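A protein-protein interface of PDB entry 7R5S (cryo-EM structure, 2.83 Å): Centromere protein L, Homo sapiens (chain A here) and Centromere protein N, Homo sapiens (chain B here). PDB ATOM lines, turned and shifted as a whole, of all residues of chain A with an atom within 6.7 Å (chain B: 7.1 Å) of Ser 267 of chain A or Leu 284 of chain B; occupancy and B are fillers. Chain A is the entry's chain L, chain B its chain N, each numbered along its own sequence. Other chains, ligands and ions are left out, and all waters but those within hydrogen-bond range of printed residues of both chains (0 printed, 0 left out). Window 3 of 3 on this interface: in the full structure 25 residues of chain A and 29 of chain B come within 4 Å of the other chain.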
ATOM      1  N   ASP A 260      -7.415  28.355 -20.002  1.00  0.00           N
ATOM      2  CA  ASP A 260      -8.120  28.720 -18.777  1.00  0.00           C
ATOM      3  C   ASP A 260      -8.478  27.484 -17.961  1.00  0.00           C
ATOM      4  O   ASP A 260      -8.358  27.487 -16.730  1.00  0.00           O
ATOM      5  CB  ASP A 260      -9.373  29.526 -19.114  1.00  0.00           C
ATOM      6  CG  ASP A 260      -9.055  30.816 -19.843  1.00  0.00           C
ATOM      7  OD1 ASP A 260      -7.862  31.073 -20.106  1.00  0.00           O
ATOM      8  OD2 ASP A 260      -9.998  31.575 -20.150  1.00  0.00           O
ATOM      9  N   LYS A 262      -6.825  24.640 -18.023  1.00  0.00           N
ATOM     10  CA  LYS A 262      -5.573  24.126 -17.475  1.00  0.00           C
ATOM     11  C   LYS A 262      -5.145  24.919 -16.248  1.00  0.00           C
ATOM     12  O   LYS A 262      -4.675  24.342 -15.259  1.00  0.00           O
ATOM     13  CB  LYS A 262      -4.481  24.159 -18.544  1.00  0.00           C
ATOM     14  CG  LYS A 262      -3.212  23.417 -18.158  1.00  0.00           C
ATOM     15  CD  LYS A 262      -3.469  21.928 -18.005  1.00  0.00           C
ATOM     16  CE  LYS A 262      -2.172  21.161 -17.808  1.00  0.00           C
ATOM     17  NZ  LYS A 262      -1.427  21.625 -16.606  1.00  0.00           N
ATOM     18  N   ALA A 263      -5.302  26.245 -16.289  1.00  0.00           N
ATOM     19  CA  ALA A 263      -4.971  27.061 -15.125  1.00  0.00           C
ATOM     20  C   ALA A 263      -5.896  26.752 -13.954  1.00  0.00           C
ATOM     21  O   ALA A 263      -5.443  26.653 -12.806  1.00  0.00           O
ATOM     22  CB  ALA A 263      -5.038  28.544 -15.487  1.00  0.00           C
ATOM     23  N   LEU A 264      -7.193  26.589 -14.225  1.00  0.00           N
ATOM     24  CA  LEU A 264      -8.137  26.261 -13.162  1.00  0.00           C
ATOM     25  C   LEU A 264      -7.827  24.902 -12.548  1.00  0.00           C
ATOM     26  O   LEU A 264      -8.004  24.701 -11.341  1.00  0.00           O
ATOM     27  CB  LEU A 264      -9.565  26.294 -13.705  1.00  0.00           C
ATOM     28  CG  LEU A 264     -10.698  26.134 -12.692  1.00  0.00           C
ATOM     29  CD1 LEU A 264     -10.660  27.255 -11.668  1.00  0.00           C
ATOM     30  CD2 LEU A 264     -12.042  26.095 -13.400  1.00  0.00           C
ATOM     31  N   TRP A 265      -7.360  23.953 -13.364  1.00  0.00           N
ATOM     32  CA  TRP A 265      -6.992  22.644 -12.835  1.00  0.00           C
ATOM     33  C   TRP A 265      -5.714  22.721 -12.010  1.00  0.00           C
ATOM     34  O   TRP A 265      -5.624  22.109 -10.939  1.00  0.00           O
ATOM     35  CB  TRP A 265      -6.833  21.641 -13.976  1.00  0.00           C
ATOM     36  CG  TRP A 265      -6.124  20.387 -13.566  1.00  0.00           C
ATOM     37  CD1 TRP A 265      -4.831  20.051 -13.836  1.00  0.00           C
ATOM     38  CD2 TRP A 265      -6.671  19.302 -12.808  1.00  0.00           C
ATOM     39  NE1 TRP A 265      -4.537  18.824 -13.295  1.00  0.00           N
ATOM     40  CE2 TRP A 265      -5.651  18.342 -12.658  1.00  0.00           C
ATOM     41  CE3 TRP A 265      -7.924  19.048 -12.241  1.00  0.00           C
ATOM     42  CZ2 TRP A 265      -5.846  17.149 -11.966  1.00  0.00           C
ATOM     43  CZ3 TRP A 265      -8.114  17.863 -11.556  1.00  0.00           C
ATOM     44  CH2 TRP A 265      -7.080  16.929 -11.423  1.00  0.00           C
ATOM     45  N   ASP A 266      -4.713  23.462 -12.493  1.00  0.00           N
ATOM     46  CA  ASP A 266      -3.472  23.606 -11.741  1.00  0.00           C
ATOM     47  C   ASP A 266      -3.688  24.359 -10.435  1.00  0.00           C
ATOM     48  O   ASP A 266      -2.918  24.180  -9.485  1.00  0.00           O
ATOM     49  CB  ASP A 266      -2.419  24.315 -12.591  1.00  0.00           C
ATOM     50  CG  ASP A 266      -1.954  23.477 -13.762  1.00  0.00           C
ATOM     51  OD1 ASP A 266      -2.403  22.318 -13.880  1.00  0.00           O
ATOM     52  OD2 ASP A 266      -1.138  23.976 -14.566  1.00  0.00           O
ATOM     53  N   SER A 267      -4.719  25.203 -10.370  1.00  0.00           N
ATOM     54  CA  SER A 267      -4.992  25.928  -9.134  1.00  0.00           C
ATOM     55  C   SER A 267      -5.445  24.998  -8.014  1.00  0.00           C
ATOM     56  O   SER A 267      -5.186  25.278  -6.839  1.00  0.00           O
ATOM     57  CB  SER A 267      -6.044  27.008  -9.381  1.00  0.00           C
ATOM     58  OG  SER A 267      -6.671  27.389  -8.169  1.00  0.00           O
ATOM     59  N   VAL A 268      -6.117  23.898  -8.349  1.00  0.00           N
ATOM     60  CA  VAL A 268      -6.634  22.970  -7.347  1.00  0.00           C
ATOM     61  C   VAL A 268      -5.828  21.685  -7.252  1.00  0.00           C
ATOM     62  O   VAL A 268      -6.043  20.908  -6.307  1.00  0.00           O
ATOM     63  CB  VAL A 268      -8.120  22.634  -7.598  1.00  0.00           C
ATOM     64  CG1 VAL A 268      -8.950  23.906  -7.650  1.00  0.00           C
ATOM     65  CG2 VAL A 268      -8.274  21.833  -8.880  1.00  0.00           C
ATOM     66  N   HIS A 269      -4.916  21.431  -8.185  1.00  0.00           N
ATOM     67  CA  HIS A 269      -4.129  20.204  -8.173  1.00  0.00           C
ATOM     68  C   HIS A 269      -3.007  20.323  -7.149  1.00  0.00           C
ATOM     69  O   HIS A 269      -2.210  21.265  -7.199  1.00  0.00           O
ATOM     70  CB  HIS A 269      -3.564  19.924  -9.564  1.00  0.00           C
ATOM     71  CG  HIS A 269      -2.877  18.600  -9.681  1.00  0.00           C
ATOM     72  ND1 HIS A 269      -3.564  17.405  -9.712  1.00  0.00           N
ATOM     73  CD2 HIS A 269      -1.565  18.281  -9.777  1.00  0.00           C
ATOM     74  CE1 HIS A 269      -2.705  16.409  -9.824  1.00  0.00           C
ATOM     75  NE2 HIS A 269      -1.485  16.913  -9.864  1.00  0.00           N
ATOM     76  N   LYS A 270      -2.944  19.367  -6.221  1.00  0.00           N
ATOM     77  CA  LYS A 270      -1.913  19.359  -5.191  1.00  0.00           C
ATOM     78  C   LYS A 270      -1.215  18.019  -5.013  1.00  0.00           C
ATOM     79  O   LYS A 270      -0.146  17.988  -4.391  1.00  0.00           O
ATOM     80  CB  LYS A 270      -2.500  19.790  -3.839  1.00  0.00           C
ATOM     81  CG  LYS A 270      -2.854  21.267  -3.765  1.00  0.00           C
ATOM     82  CD  LYS A 270      -3.396  21.642  -2.397  1.00  0.00           C
ATOM     83  CE  LYS A 270      -3.612  23.142  -2.283  1.00  0.00           C
ATOM     84  NZ  LYS A 270      -4.530  23.651  -3.338  1.00  0.00           N
ATOM     85  N   CYS A 286     -15.865  24.309  -8.999  1.00  0.00           N
ATOM     86  CA  CYS A 286     -15.456  25.604  -9.536  1.00  0.00           C
ATOM     87  C   CYS A 286     -16.361  26.028 -10.688  1.00  0.00           C
ATOM     88  O   CYS A 286     -16.879  27.153 -10.708  1.00  0.00           O
ATOM     89  CB  CYS A 286     -13.996  25.549  -9.988  1.00  0.00           C
ATOM     90  SG  CYS A 286     -12.799  25.457  -8.637  1.00  0.00           S
ATOM     91  N   LYS B 274     -14.252  37.948 -14.756  1.00  0.00           N
ATOM     92  CA  LYS B 274     -13.208  37.375 -13.921  1.00  0.00           C
ATOM     93  C   LYS B 274     -13.783  36.318 -12.986  1.00  0.00           C
ATOM     94  O   LYS B 274     -14.948  36.380 -12.584  1.00  0.00           O
ATOM     95  CB  LYS B 274     -12.511  38.465 -13.105  1.00  0.00           C
ATOM     96  CG  LYS B 274     -11.856  39.545 -13.947  1.00  0.00           C
ATOM     97  CD  LYS B 274     -11.337  40.680 -13.079  1.00  0.00           C
ATOM     98  CE  LYS B 274     -10.338  40.176 -12.051  1.00  0.00           C
ATOM     99  NZ  LYS B 274      -9.155  39.544 -12.695  1.00  0.00           N
ATOM    100  N   PHE B 275     -12.946  35.344 -12.640  1.00  0.00           N
ATOM    101  CA  PHE B 275     -13.336  34.283 -11.720  1.00  0.00           C
ATOM    102  C   PHE B 275     -13.151  34.765 -10.286  1.00  0.00           C
ATOM    103  O   PHE B 275     -12.032  35.089  -9.873  1.00  0.00           O
ATOM    104  CB  PHE B 275     -12.511  33.025 -11.982  1.00  0.00           C
ATOM    105  CG  PHE B 275     -12.869  31.868 -11.094  1.00  0.00           C
ATOM    106  CD1 PHE B 275     -13.994  31.103 -11.350  1.00  0.00           C
ATOM    107  CD2 PHE B 275     -12.074  31.538 -10.009  1.00  0.00           C
ATOM    108  CE1 PHE B 275     -14.325  30.037 -10.537  1.00  0.00           C
ATOM    109  CE2 PHE B 275     -12.399  30.472  -9.193  1.00  0.00           C
ATOM    110  CZ  PHE B 275     -13.526  29.721  -9.458  1.00  0.00           C
ATOM    111  N   LYS B 276     -14.244  34.813  -9.529  1.00  0.00           N
ATOM    112  CA  LYS B 276     -14.237  35.299  -8.150  1.00  0.00           C
ATOM    113  C   LYS B 276     -14.819  34.210  -7.254  1.00  0.00           C
ATOM    114  O   LYS B 276     -16.037  34.010  -7.220  1.00  0.00           O
ATOM    115  CB  LYS B 276     -15.023  36.601  -8.024  1.00  0.00           C
ATOM    116  N   SER B 277     -13.949  33.513  -6.531  1.00  0.00           N
ATOM    117  CA  SER B 277     -14.380  32.463  -5.616  1.00  0.00           C
ATOM    118  C   SER B 277     -13.364  32.262  -4.498  1.00  0.00           C
ATOM    119  O   SER B 277     -12.161  32.424  -4.704  1.00  0.00           O
ATOM    120  CB  SER B 277     -14.598  31.150  -6.370  1.00  0.00           C
ATOM    121  N   SER B 282      -8.161  32.570  -2.704  1.00  0.00           N
ATOM    122  CA  SER B 282      -7.839  31.174  -2.435  1.00  0.00           C
ATOM    123  C   SER B 282      -7.623  30.401  -3.733  1.00  0.00           C
ATOM    124  O   SER B 282      -6.642  29.671  -3.875  1.00  0.00           O
ATOM    125  CB  SER B 282      -8.947  30.517  -1.610  1.00  0.00           C
ATOM    126  OG  SER B 282     -10.228  30.857  -2.113  1.00  0.00           O
ATOM    127  N   ILE B 283      -8.544  30.569  -4.678  1.00  0.00           N
ATOM    128  CA  ILE B 283      -8.485  29.906  -5.976  1.00  0.00           C
ATOM    129  C   ILE B 283      -8.411  30.990  -7.042  1.00  0.00           C
ATOM    130  O   ILE B 283      -9.376  31.741  -7.239  1.00  0.00           O
ATOM    131  CB  ILE B 283      -9.687  28.981  -6.208  1.00  0.00           C
ATOM    132  CG1 ILE B 283      -9.673  27.827  -5.205  1.00  0.00           C
ATOM    133  CG2 ILE B 283      -9.689  28.455  -7.634  1.00  0.00           C
ATOM    134  CD1 ILE B 283     -10.810  26.845  -5.386  1.00  0.00           C
ATOM    135  N   LEU B 284      -7.268  31.071  -7.726  1.00  0.00           N
ATOM    136  CA  LEU B 284      -7.044  32.049  -8.793  1.00  0.00           C
ATOM    137  C   LEU B 284      -7.254  33.477  -8.298  1.00  0.00           C
ATOM    138  O   LEU B 284      -7.803  34.326  -9.004  1.00  0.00           O
ATOM    139  CB  LEU B 284      -7.931  31.757 -10.007  1.00  0.00           C
ATOM    140  CG  LEU B 284      -7.605  30.486 -10.791  1.00  0.00           C
ATOM    141  CD1 LEU B 284      -8.534  30.337 -11.983  1.00  0.00           C
ATOM    142  CD2 LEU B 284      -6.152  30.492 -11.237  1.00  0.00           C
ATOM    143  N   ALA B 285      -6.809  33.748  -7.069  1.00  0.00           N
ATOM    144  CA  ALA B 285      -6.935  35.095  -6.522  1.00  0.00           C
ATOM    145  C   ALA B 285      -5.938  36.054  -7.157  1.00  0.00           C
ATOM    146  O   ALA B 285      -6.253  37.234  -7.352  1.00  0.00           O
ATOM    147  CB  ALA B 285      -6.752  35.066  -5.005  1.00  0.00           C
ATOM    148  N   GLU B 286      -4.739  35.574  -7.487  1.00  0.00           N
ATOM    149  CA  GLU B 286      -3.720  36.414  -8.103  1.00  0.00           C
ATOM    150  C   GLU B 286      -3.942  36.625  -9.594  1.00  0.00           C
ATOM    151  O   GLU B 286      -3.285  37.490 -10.183  1.00  0.00           O
ATOM    152  CB  GLU B 286      -2.331  35.809  -7.876  1.00  0.00           C
ATOM    153  CG  GLU B 286      -2.054  34.543  -8.676  1.00  0.00           C
ATOM    154  CD  GLU B 286      -2.708  33.312  -8.078  1.00  0.00           C
ATOM    155  OE1 GLU B 286      -3.175  33.386  -6.922  1.00  0.00           O
ATOM    156  OE2 GLU B 286      -2.754  32.270  -8.764  1.00  0.00           O
ATOM    157  N   ARG B 287      -4.840  35.864 -10.214  1.00  0.00           N
ATOM    158  CA  ARG B 287      -5.087  36.006 -11.643  1.00  0.00           C
ATOM    159  C   ARG B 287      -5.772  37.335 -11.934  1.00  0.00           C
ATOM    160  O   ARG B 287      -6.742  37.706 -11.265  1.00  0.00           O
ATOM    161  CB  ARG B 287      -5.943  34.846 -12.149  1.00  0.00           C
ATOM    162  CG  ARG B 287      -6.189  34.862 -13.647  1.00  0.00           C
ATOM    163  CD  ARG B 287      -7.051  33.685 -14.077  1.00  0.00           C
ATOM    164  NE  ARG B 287      -7.264  33.658 -15.520  1.00  0.00           N
ATOM    165  CZ  ARG B 287      -6.465  33.035 -16.381  1.00  0.00           C
ATOM    166  NH1 ARG B 287      -5.395  32.385 -15.945  1.00  0.00           N
ATOM    167  NH2 ARG B 287      -6.736  33.062 -17.679  1.00  0.00           N
ATOM    168  N   GLU B 288      -5.263  38.052 -12.934  1.00  0.00           N
ATOM    169  CA  GLU B 288      -5.815  39.338 -13.338  1.00  0.00           C
ATOM    170  C   GLU B 288      -6.415  39.299 -14.738  1.00  0.00           C
ATOM    171  O   GLU B 288      -6.800  40.348 -15.268  1.00  0.00           O
ATOM    172  CB  GLU B 288      -4.739  40.424 -13.260  1.00  0.00           C
ATOM    173  N   LEU B 291     -11.934  35.142 -17.715  1.00  0.00           N
ATOM    174  CA  LEU B 291     -12.199  33.761 -18.099  1.00  0.00           C
ATOM    175  C   LEU B 291     -13.135  33.776 -19.301  1.00  0.00           C
ATOM    176  O   LEU B 291     -14.311  34.137 -19.175  1.00  0.00           O
ATOM    177  CB  LEU B 291     -12.806  32.980 -16.935  1.00  0.00           C
ATOM    178  CG  LEU B 291     -12.351  31.531 -16.755  1.00  0.00           C
ATOM    179  CD1 LEU B 291     -10.885  31.478 -16.365  1.00  0.00           C
ATOM    180  CD2 LEU B 291     -13.210  30.825 -15.718  1.00  0.00           C
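NH2 of Arg 287 of chain B lies within salt-bridge range of OD1 of Asp 260 of chain A.
The side-chain amino group of Lys 274 of chain B sits at hydrogen-bond distance from the backbone carbonyl oxygen of Arg 287 of chain B, 3.4 Å away.
Among the printed residues, pairs that only touch across the chains: Asp 260 of chain A with Leu 291 of chain B, Ala 263 of chain A with Arg 287 of chain B, Leu 264 of chain A with Leu 284 of chain B, Ser 267 of chain A with Ile 283 of chain B, Ser 267 of chain A with Leu 284 of chain B and Cys 286 of chain A with Phe 275 of chain B.
Ser 267 of chain A touches just these residues of chain B: Ile 283 (3.2 Å) and Leu 284 (3.8 Å). Of the printed residues of chain A, Ile 283 of chain B touches Ser 267 (3.2 Å). Of the printed residues of chain A, Leu 291 of chain B touches Asp 260 (3.7 Å). Of the printed residues of chain A, Phe 275 of chain B touches Cys 286 (3.9 Å). Lys 270 of chain A touches none of the printed residues of chain B. The nearest residue of chain B that does not touch Ser 267 of chain A is Ser 282 of chain B (4.9 Å).
Hydrophobic or aromatic side chains of chain B within 4 Å of the printed part of chain A: Phe 275, Ile 283, Leu 284 and Leu 291. Among the printed residues, 7 pairs touch across the chains.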
